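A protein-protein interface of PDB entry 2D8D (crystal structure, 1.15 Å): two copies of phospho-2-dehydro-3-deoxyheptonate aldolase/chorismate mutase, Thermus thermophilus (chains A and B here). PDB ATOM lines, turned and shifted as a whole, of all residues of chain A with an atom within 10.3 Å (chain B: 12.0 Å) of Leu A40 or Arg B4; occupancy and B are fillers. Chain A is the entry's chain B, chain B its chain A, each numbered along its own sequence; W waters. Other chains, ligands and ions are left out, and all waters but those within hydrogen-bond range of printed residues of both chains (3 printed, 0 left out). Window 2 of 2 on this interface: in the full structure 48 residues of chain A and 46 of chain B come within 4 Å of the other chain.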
ATOM      1  N   LEU A  29     -12.710 -13.712  -3.346  1.00  0.00           N
ATOM      2  CA  LEU A  29     -11.894 -14.371  -4.358  1.00  0.00           C
ATOM      3  C   LEU A  29     -10.618 -14.943  -3.754  1.00  0.00           C
ATOM      4  O   LEU A  29     -10.246 -16.087  -4.030  1.00  0.00           O
ATOM      5  CB  LEU A  29     -11.534 -13.388  -5.474  1.00  0.00           C
ATOM      6  CG  LEU A  29     -12.659 -13.021  -6.440  1.00  0.00           C
ATOM      7  CD1 LEU A  29     -12.223 -11.855  -7.309  1.00  0.00           C
ATOM      8  CD2 LEU A  29     -13.016 -14.229  -7.297  1.00  0.00           C
ATOM      9  N   VAL A  30      -9.941 -14.153  -2.932  1.00  0.00           N
ATOM     10  CA  VAL A  30      -8.713 -14.622  -2.312  1.00  0.00           C
ATOM     11  C   VAL A  30      -9.013 -15.743  -1.322  1.00  0.00           C
ATOM     12  O   VAL A  30      -8.185 -16.626  -1.117  1.00  0.00           O
ATOM     13  CB  VAL A  30      -7.960 -13.467  -1.627  1.00  0.00           C
ATOM     14  CG1 VAL A  30      -7.340 -12.561  -2.679  1.00  0.00           C
ATOM     15  CG2 VAL A  30      -8.908 -12.673  -0.773  1.00  0.00           C
ATOM     16  N   GLU A  32     -11.234 -18.008  -1.784  1.00  0.00           N
ATOM     17  CA  GLU A  32     -11.381 -19.175  -2.638  1.00  0.00           C
ATOM     18  C   GLU A  32     -10.012 -19.685  -3.074  1.00  0.00           C
ATOM     19  O   GLU A  32      -9.768 -20.894  -3.097  1.00  0.00           O
ATOM     20  CB  GLU A  32     -12.227 -18.827  -3.862  1.00  0.00           C
ATOM     21  CG  GLU A  32     -12.953 -20.014  -4.460  1.00  0.00           C
ATOM     22  CD  GLU A  32     -13.858 -19.619  -5.604  1.00  0.00           C
ATOM     23  OE1 GLU A  32     -14.483 -18.541  -5.516  1.00  0.00           O
ATOM     24  OE2 GLU A  32     -13.953 -20.389  -6.580  1.00  0.00           O
ATOM     25  N   ILE A  33      -9.120 -18.766  -3.429  1.00  0.00           N
ATOM     26  CA  ILE A  33      -7.774 -19.148  -3.837  1.00  0.00           C
ATOM     27  C   ILE A  33      -7.073 -19.821  -2.658  1.00  0.00           C
ATOM     28  O   ILE A  33      -6.423 -20.855  -2.815  1.00  0.00           O
ATOM     29  CB  ILE A  33      -6.954 -17.912  -4.282  1.00  0.00           C
ATOM     30  CG1 ILE A  33      -7.502 -17.372  -5.609  1.00  0.00           C
ATOM     31  CG2 ILE A  33      -5.480 -18.279  -4.402  1.00  0.00           C
ATOM     32  CD1 ILE A  33      -6.935 -16.023  -6.010  1.00  0.00           C
ATOM     33  N   GLY A  34      -7.227 -19.238  -1.474  1.00  0.00           N
ATOM     34  CA  GLY A  34      -6.599 -19.784  -0.282  1.00  0.00           C
ATOM     35  C   GLY A  34      -7.027 -21.201   0.043  1.00  0.00           C
ATOM     36  O   GLY A  34      -6.203 -22.020   0.452  1.00  0.00           O
ATOM     37  N   ARG A  35      -8.313 -21.492  -0.133  1.00  0.00           N
ATOM     38  CA  ARG A  35      -8.838 -22.823   0.139  1.00  0.00           C
ATOM     39  C   ARG A  35      -8.216 -23.824  -0.828  1.00  0.00           C
ATOM     40  O   ARG A  35      -7.866 -24.941  -0.441  1.00  0.00           O
ATOM     41  CB  ARG A  35     -10.363 -22.825   0.003  1.00  0.00           C
ATOM     42  CG  ARG A  35     -11.088 -22.034   1.083  1.00  0.00           C
ATOM     43  CD  ARG A  35     -11.221 -22.832   2.371  1.00  0.00           C
ATOM     44  NE  ARG A  35     -12.243 -23.872   2.267  1.00  0.00           N
ATOM     45  CZ  ARG A  35     -13.552 -23.636   2.220  1.00  0.00           C
ATOM     46  NH1 ARG A  35     -14.008 -22.392   2.273  1.00  0.00           N
ATOM     47  NH2 ARG A  35     -14.408 -24.644   2.121  1.00  0.00           N
ATOM     48  N   LEU A  36      -8.071 -23.425  -2.086  1.00  0.00           N
ATOM     49  CA  LEU A  36      -7.470 -24.300  -3.084  1.00  0.00           C
ATOM     50  C   LEU A  36      -5.997 -24.534  -2.777  1.00  0.00           C
ATOM     51  O   LEU A  36      -5.502 -25.654  -2.902  1.00  0.00           O
ATOM     52  CB  LEU A  36      -7.618 -23.703  -4.485  1.00  0.00           C
ATOM     53  CG  LEU A  36      -9.032 -23.754  -5.068  1.00  0.00           C
ATOM     54  CD1 LEU A  36      -9.074 -22.996  -6.382  1.00  0.00           C
ATOM     55  CD2 LEU A  36      -9.457 -25.201  -5.267  1.00  0.00           C
ATOM     56  N   GLN A  37      -5.295 -23.480  -2.375  1.00  0.00           N
ATOM     57  CA  GLN A  37      -3.882 -23.615  -2.055  1.00  0.00           C
ATOM     58  C   GLN A  37      -3.690 -24.556  -0.873  1.00  0.00           C
ATOM     59  O   GLN A  37      -2.782 -25.382  -0.876  1.00  0.00           O
ATOM     60  CB  GLN A  37      -3.277 -22.242  -1.766  1.00  0.00           C
ATOM     61  CG  GLN A  37      -3.260 -21.350  -3.001  1.00  0.00           C
ATOM     62  CD  GLN A  37      -2.813 -19.939  -2.710  1.00  0.00           C
ATOM     63  OE1 GLN A  37      -3.201 -19.354  -1.705  1.00  0.00           O
ATOM     64  NE2 GLN A  37      -2.005 -19.376  -3.603  1.00  0.00           N
ATOM     65  N   THR A  38      -4.554 -24.444   0.129  1.00  0.00           N
ATOM     66  CA  THR A  38      -4.457 -25.312   1.295  1.00  0.00           C
ATOM     67  C   THR A  38      -4.641 -26.776   0.913  1.00  0.00           C
ATOM     68  O   THR A  38      -3.870 -27.634   1.339  1.00  0.00           O
ATOM     69  CB  THR A  38      -5.505 -24.934   2.362  1.00  0.00           C
ATOM     70  OG1 THR A  38      -5.146 -23.680   2.953  1.00  0.00           O
ATOM     71  CG2 THR A  38      -5.579 -26.005   3.448  1.00  0.00           C
ATOM     72  N   GLU A  39      -5.652 -27.066   0.101  1.00  0.00           N
ATOM     73  CA  GLU A  39      -5.907 -28.444  -0.299  1.00  0.00           C
ATOM     74  C   GLU A  39      -4.826 -28.991  -1.226  1.00  0.00           C
ATOM     75  O   GLU A  39      -4.563 -30.193  -1.238  1.00  0.00           O
ATOM     76  CB  GLU A  39      -7.275 -28.564  -0.975  1.00  0.00           C
ATOM     77  CG  GLU A  39      -7.778 -30.000  -1.056  1.00  0.00           C
ATOM     78  CD  GLU A  39      -9.174 -30.110  -1.637  1.00  0.00           C
ATOM     79  OE1 GLU A  39     -10.084 -29.411  -1.144  1.00  0.00           O
ATOM     80  OE2 GLU A  39      -9.361 -30.904  -2.583  1.00  0.00           O
ATOM     81  N   LEU A  40      -4.190 -28.108  -1.990  1.00  0.00           N
ATOM     82  CA  LEU A  40      -3.144 -28.523  -2.918  1.00  0.00           C
ATOM     83  C   LEU A  40      -1.756 -28.502  -2.284  1.00  0.00           C
ATOM     84  O   LEU A  40      -0.771 -28.878  -2.921  1.00  0.00           O
ATOM     85  CB  LEU A  40      -3.155 -27.623  -4.156  1.00  0.00           C
ATOM     86  CG  LEU A  40      -4.405 -27.684  -5.037  1.00  0.00           C
ATOM     87  CD1 LEU A  40      -4.336 -26.587  -6.084  1.00  0.00           C
ATOM     88  CD2 LEU A  40      -4.518 -29.054  -5.695  1.00  0.00           C
ATOM     89  N   GLY A  41      -1.679 -28.065  -1.030  1.00  0.00           N
ATOM     90  CA  GLY A  41      -0.401 -28.007  -0.342  1.00  0.00           C
ATOM     91  C   GLY A  41       0.511 -26.930  -0.899  1.00  0.00           C
ATOM     92  O   GLY A  41       1.728 -27.108  -0.961  1.00  0.00           O
ATOM     93  N   LEU A  42      -0.078 -25.808  -1.300  1.00  0.00           N
ATOM     94  CA  LEU A  42       0.677 -24.694  -1.859  1.00  0.00           C
ATOM     95  C   LEU A  42       0.733 -23.534  -0.874  1.00  0.00           C
ATOM     96  O   LEU A  42      -0.128 -23.405  -0.004  1.00  0.00           O
ATOM     97  CB  LEU A  42       0.024 -24.219  -3.160  1.00  0.00           C
ATOM     98  CG  LEU A  42      -0.159 -25.251  -4.275  1.00  0.00           C
ATOM     99  CD1 LEU A  42      -0.947 -24.631  -5.419  1.00  0.00           C
ATOM    100  CD2 LEU A  42       1.199 -25.737  -4.757  1.00  0.00           C
ATOM    101  N   PRO A  43       1.752 -22.671  -0.994  1.00  0.00           N
ATOM    102  CA  PRO A  43       1.876 -21.526  -0.090  1.00  0.00           C
ATOM    103  C   PRO A  43       0.839 -20.444  -0.400  1.00  0.00           C
ATOM    104  O   PRO A  43       0.343 -20.357  -1.522  1.00  0.00           O
ATOM    105  CB  PRO A  43       3.305 -21.053  -0.339  1.00  0.00           C
ATOM    106  CG  PRO A  43       3.499 -21.358  -1.791  1.00  0.00           C
ATOM    107  CD  PRO A  43       2.903 -22.744  -1.912  1.00  0.00           C
ATOM    108  N   HIS A  44       0.511 -19.634   0.602  1.00  0.00           N
ATOM    109  CA  HIS A  44      -0.457 -18.549   0.447  1.00  0.00           C
ATOM    110  C   HIS A  44       0.247 -17.247   0.073  1.00  0.00           C
ATOM    111  O   HIS A  44      -0.268 -16.452  -0.714  1.00  0.00           O
ATOM    112  CB  HIS A  44      -1.229 -18.343   1.754  1.00  0.00           C
ATOM    113  CG  HIS A  44      -2.229 -19.416   2.043  1.00  0.00           C
ATOM    114  ND1 HIS A  44      -2.512 -19.843   3.324  1.00  0.00           N
ATOM    115  CD2 HIS A  44      -3.047 -20.121   1.227  1.00  0.00           C
ATOM    116  CE1 HIS A  44      -3.457 -20.762   3.281  1.00  0.00           C
ATOM    117  NE2 HIS A  44      -3.800 -20.951   2.019  1.00  0.00           N
ATOM    118  N   ARG A  49       3.832 -12.721  -7.261  1.00  0.00           N
ATOM    119  CA  ARG A  49       2.489 -12.334  -7.683  1.00  0.00           C
ATOM    120  C   ARG A  49       2.151 -10.931  -7.179  1.00  0.00           C
ATOM    121  O   ARG A  49       1.600 -10.111  -7.917  1.00  0.00           O
ATOM    122  CB  ARG A  49       1.483 -13.362  -7.154  1.00  0.00           C
ATOM    123  CG  ARG A  49       0.021 -12.957  -7.210  1.00  0.00           C
ATOM    124  CD  ARG A  49      -0.490 -12.699  -8.618  1.00  0.00           C
ATOM    125  NE  ARG A  49      -1.938 -12.516  -8.582  1.00  0.00           N
ATOM    126  CZ  ARG A  49      -2.670 -11.988  -9.556  1.00  0.00           C
ATOM    127  NH1 ARG A  49      -2.101 -11.574 -10.680  1.00  0.00           N
ATOM    128  NH2 ARG A  49      -3.980 -11.863  -9.395  1.00  0.00           N
ATOM    129  N   GLU B   3      -4.826 -22.914 -14.438  1.00  0.00           N
ATOM    130  CA  GLU B   3      -5.740 -23.817 -13.681  1.00  0.00           C
ATOM    131  C   GLU B   3      -6.853 -23.032 -12.999  1.00  0.00           C
ATOM    132  O   GLU B   3      -7.218 -21.945 -13.444  1.00  0.00           O
ATOM    133  CB  GLU B   3      -4.945 -24.608 -12.639  1.00  0.00           C
ATOM    134  CG  GLU B   3      -4.124 -23.746 -11.690  1.00  0.00           C
ATOM    135  CD  GLU B   3      -3.294 -24.567 -10.719  1.00  0.00           C
ATOM    136  OE1 GLU B   3      -3.882 -25.233  -9.841  1.00  0.00           O
ATOM    137  OE2 GLU B   3      -2.050 -24.548 -10.834  1.00  0.00           O
ATOM    138  N   ARG B   4      -7.395 -23.592 -11.923  1.00  0.00           N
ATOM    139  CA  ARG B   4      -8.463 -22.935 -11.181  1.00  0.00           C
ATOM    140  C   ARG B   4      -7.921 -21.696 -10.479  1.00  0.00           C
ATOM    141  O   ARG B   4      -8.571 -20.649 -10.461  1.00  0.00           O
ATOM    142  CB  ARG B   4      -9.064 -23.899 -10.158  1.00  0.00           C
ATOM    143  CG  ARG B   4      -9.729 -25.116 -10.780  1.00  0.00           C
ATOM    144  CD  ARG B   4     -10.055 -26.152  -9.723  1.00  0.00           C
ATOM    145  NE  ARG B   4      -8.842 -26.722  -9.148  1.00  0.00           N
ATOM    146  CZ  ARG B   4      -8.830 -27.614  -8.162  1.00  0.00           C
ATOM    147  NH1 ARG B   4      -9.969 -28.040  -7.635  1.00  0.00           N
ATOM    148  NH2 ARG B   4      -7.677 -28.081  -7.706  1.00  0.00           N
ATOM    149  N   ILE B   5      -6.734 -21.814  -9.895  1.00  0.00           N
ATOM    150  CA  ILE B   5      -6.124 -20.677  -9.224  1.00  0.00           C
ATOM    151  C   ILE B   5      -5.783 -19.615 -10.265  1.00  0.00           C
ATOM    152  O   ILE B   5      -5.979 -18.423 -10.029  1.00  0.00           O
ATOM    153  CB  ILE B   5      -4.853 -21.094  -8.455  1.00  0.00           C
ATOM    154  CG1 ILE B   5      -5.242 -21.974  -7.265  1.00  0.00           C
ATOM    155  CG2 ILE B   5      -4.093 -19.858  -7.983  1.00  0.00           C
ATOM    156  CD1 ILE B   5      -4.075 -22.464  -6.441  1.00  0.00           C
ATOM    157  N   GLN B   6      -5.285 -20.047 -11.420  1.00  0.00           N
ATOM    158  CA  GLN B   6      -4.943 -19.113 -12.484  1.00  0.00           C
ATOM    159  C   GLN B   6      -6.191 -18.351 -12.918  1.00  0.00           C
ATOM    160  O   GLN B   6      -6.138 -17.145 -13.164  1.00  0.00           O
ATOM    161  CB  GLN B   6      -4.351 -19.856 -13.684  1.00  0.00           C
ATOM    162  CG  GLN B   6      -3.948 -18.938 -14.830  1.00  0.00           C
ATOM    163  CD  GLN B   6      -3.344 -19.687 -16.002  1.00  0.00           C
ATOM    164  OE1 GLN B   6      -3.196 -20.910 -15.960  1.00  0.00           O
ATOM    165  NE2 GLN B   6      -2.991 -18.960 -17.056  1.00  0.00           N
ATOM    166  N   ALA B   7      -7.315 -19.057 -13.006  1.00  0.00           N
ATOM    167  CA  ALA B   7      -8.574 -18.438 -13.405  1.00  0.00           C
ATOM    168  C   ALA B   7      -9.023 -17.416 -12.366  1.00  0.00           C
ATOM    169  O   ALA B   7      -9.448 -16.313 -12.711  1.00  0.00           O
ATOM    170  CB  ALA B   7      -9.647 -19.506 -13.592  1.00  0.00           C
ATOM    171  N   LEU B   8      -8.925 -17.780 -11.092  1.00  0.00           N
ATOM    172  CA  LEU B   8      -9.320 -16.876 -10.020  1.00  0.00           C
ATOM    173  C   LEU B   8      -8.420 -15.644  -9.980  1.00  0.00           C
ATOM    174  O   LEU B   8      -8.881 -14.544  -9.671  1.00  0.00           O
ATOM    175  CB  LEU B   8      -9.283 -17.607  -8.675  1.00  0.00           C
ATOM    176  CG  LEU B   8     -10.403 -18.633  -8.464  1.00  0.00           C
ATOM    177  CD1 LEU B   8     -10.082 -19.526  -7.276  1.00  0.00           C
ATOM    178  CD2 LEU B   8     -11.724 -17.907  -8.265  1.00  0.00           C
ATOM    179  N   ARG B   9      -7.140 -15.821 -10.292  1.00  0.00           N
ATOM    180  CA  ARG B   9      -6.220 -14.692 -10.297  1.00  0.00           C
ATOM    181  C   ARG B   9      -6.620 -13.683 -11.371  1.00  0.00           C
ATOM    182  O   ARG B   9      -6.425 -12.479 -11.198  1.00  0.00           O
ATOM    183  CB  ARG B   9      -4.779 -15.166 -10.506  1.00  0.00           C
ATOM    184  CG  ARG B   9      -4.158 -15.771  -9.251  1.00  0.00           C
ATOM    185  CD  ARG B   9      -2.676 -16.056  -9.433  1.00  0.00           C
ATOM    186  NE  ARG B   9      -2.028 -16.422  -8.175  1.00  0.00           N
ATOM    187  CZ  ARG B   9      -0.720 -16.621  -8.042  1.00  0.00           C
ATOM    188  NH1 ARG B   9       0.081 -16.492  -9.090  1.00  0.00           N
ATOM    189  NH2 ARG B   9      -0.211 -16.940  -6.860  1.00  0.00           N
ATOM    190  N   LYS B  10      -7.185 -14.168 -12.473  1.00  0.00           N
ATOM    191  CA  LYS B  10      -7.635 -13.278 -13.539  1.00  0.00           C
ATOM    192  C   LYS B  10      -8.784 -12.429 -13.006  1.00  0.00           C
ATOM    193  O   LYS B  10      -8.901 -11.247 -13.331  1.00  0.00           O
ATOM    194  CB  LYS B  10      -8.110 -14.078 -14.752  1.00  0.00           C
ATOM    195  CG  LYS B  10      -7.021 -14.407 -15.759  1.00  0.00           C
ATOM    196  CD  LYS B  10      -7.588 -15.173 -16.947  1.00  0.00           C
ATOM    197  CE  LYS B  10      -8.682 -14.398 -17.675  1.00  0.00           C
ATOM    198  NZ  LYS B  10      -8.168 -13.190 -18.378  1.00  0.00           N
ATOM    199  N   GLU B  11      -9.640 -13.037 -12.193  1.00  0.00           N
ATOM    200  CA  GLU B  11     -10.753 -12.308 -11.610  1.00  0.00           C
ATOM    201  C   GLU B  11     -10.227 -11.283 -10.616  1.00  0.00           C
ATOM    202  O   GLU B  11     -10.755 -10.174 -10.513  1.00  0.00           O
ATOM    203  CB  GLU B  11     -11.713 -13.272 -10.922  1.00  0.00           C
ATOM    204  CG  GLU B  11     -12.423 -14.175 -11.905  1.00  0.00           C
ATOM    205  CD  GLU B  11     -13.193 -13.393 -12.949  1.00  0.00           C
ATOM    206  OE1 GLU B  11     -14.054 -12.572 -12.564  1.00  0.00           O
ATOM    207  OE2 GLU B  11     -12.936 -13.599 -14.153  1.00  0.00           O
ATOM    208  N   VAL B  12      -9.179 -11.650  -9.886  1.00  0.00           N
ATOM    209  CA  VAL B  12      -8.584 -10.729  -8.931  1.00  0.00           C
ATOM    210  C   VAL B  12      -7.993  -9.543  -9.695  1.00  0.00           C
ATOM    211  O   VAL B  12      -8.114  -8.401  -9.252  1.00  0.00           O
ATOM    212  CB  VAL B  12      -7.488 -11.415  -8.078  1.00  0.00           C
ATOM    213  CG1 VAL B  12      -6.696 -10.369  -7.308  1.00  0.00           C
ATOM    214  CG2 VAL B  12      -8.131 -12.393  -7.102  1.00  0.00           C
ATOM    215  N   ASP B  13      -7.370  -9.802 -10.844  1.00  0.00           N
ATOM    216  CA  ASP B  13      -6.799  -8.720 -11.651  1.00  0.00           C
ATOM    217  C   ASP B  13      -7.895  -7.727 -12.037  1.00  0.00           C
ATOM    218  O   ASP B  13      -7.708  -6.511 -11.962  1.00  0.00           O
ATOM    219  CB  ASP B  13      -6.177  -9.252 -12.948  1.00  0.00           C
ATOM    220  CG  ASP B  13      -4.905 -10.044 -12.723  1.00  0.00           C
ATOM    221  OD1 ASP B  13      -4.232  -9.843 -11.692  1.00  0.00           O
ATOM    222  OD2 ASP B  13      -4.570 -10.858 -13.610  1.00  0.00           O
HETATM  223  O   HOH W   1     -10.825 -29.061  -4.791  1.00  0.00           O
HETATM  224  O   HOH W   2      -1.048 -16.506  -3.630  1.00  0.00           O
HETATM  225  O   HOH W   3      -3.426 -13.345 -13.382  1.00  0.00           O
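Water W3 bridges OD2 of Asp B13 (2.7 Å) and NH1 of Arg A49 (3.5 Å).
Water W2 lies within hydrogen-bond range of O of His A44 (3.0 Å), NE2 of Gln A37 (3.0 Å) and NH2 of Arg B9 (3.4 Å).
Water W1 lies within hydrogen-bond range of NH1 of Arg B4 (3.1 Å) and OE2 of Glu A39 (3.2 Å).
OD1 of Asp B13 is in salt-bridge range of NH1 of Arg A49 (2.9 Å).
The backbone carbonyl oxygen of Arg B9 sits at hydrogen-bond distance from the guanidinium group of Arg A49, at 3.1 Å.
Of the 16 printed residues of chain A, 8 touch a printed residue of chain B.
Printed residues of chain A that touch a printed residue of chain B: Leu A29, Glu A32, Ile A33, Leu A36, Gln A37, Leu A40, Leu A42 and Arg A49.
Of the 11 printed residues of chain B, 7 touch a printed residue of chain A.
Printed residues of chain B that touch a printed residue of chain A: Arg B4, Ile B5, Leu B8, Arg B9, Glu B11, Val B12 and Asp B13.
Along chain B the printed residues that touch a printed residue of chain A span positions 4 to 13.
Among the printed residues, Asp or Glu carboxylates within 4 Å of a Lys or Arg side-chain nitrogen of the other chain: Arg A49 with Asp B13 (2.9 Å).
Among the printed residues, merely in contact across the chains: Ile A33 with Leu B8, Gln A37 with Ile B5, Leu A36 with Leu B8, Leu A36 with Arg B4, Arg A49 with Val B12, Glu A32 with Leu B8, Leu A40 with Arg B4, Leu A29 with Val B12, Leu A29 with Glu B11, Leu A42 with Ile B5 and Ile A33 with Val B12.
The backbone carbonyl oxygen (O) of Gln A37 lies within hydrogen-bond range of the backbone NH (N) of Leu A42 (2.8 Å).
The side-chain amide nitrogen (NE2) of Gln A37 sits at hydrogen-bond distance from the backbone carbonyl oxygen (O) of Pro A43 (3.3 Å).
No position is printed for both chains.
Printed residues of chain B within 4 Å of Glu A32: Leu B8 (3.7 Å).
Printed residues of chain B within 4 Å of Ile A33: Leu B8 (3.6 Å) and Val B12 (3.97 Å).
Of chain B, only Arg B4 and Leu B8 come within 4 Å of Leu A36.
No residue of chain B comes within 4 Å of Thr A38.
No residue of chain B comes within 4 Å of Glu A39.
Of the printed residues of chain B, Leu A40 touches Arg B4 (3.9 Å).
No residue of chain B comes within 4 Å of Gly A41.
Leu A42 touches just one residue of chain B: Ile B5 (3.9 Å).
His A44 touches none of the printed residues of chain B.
Printed residues of chain B within 4 Å of Arg A49: Arg B9, Val B12 and Asp B13.
Arg B4 touches just these residues of chain A: Leu A36 and Leu A40.
Of the printed residues of chain A, Ile B5 touches Gln A37 and Leu A42.
No residue of chain A comes within 4 Å of Ala B7.
Printed residues of chain A within 4 Å of Val B12: Leu A29 (3.9 Å), Ile A33 (3.97 Å) and Arg A49 (3.7 Å).
The nearest printed residue of chain A that does not touch Arg B9 is Ile A33 (4.3 Å).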
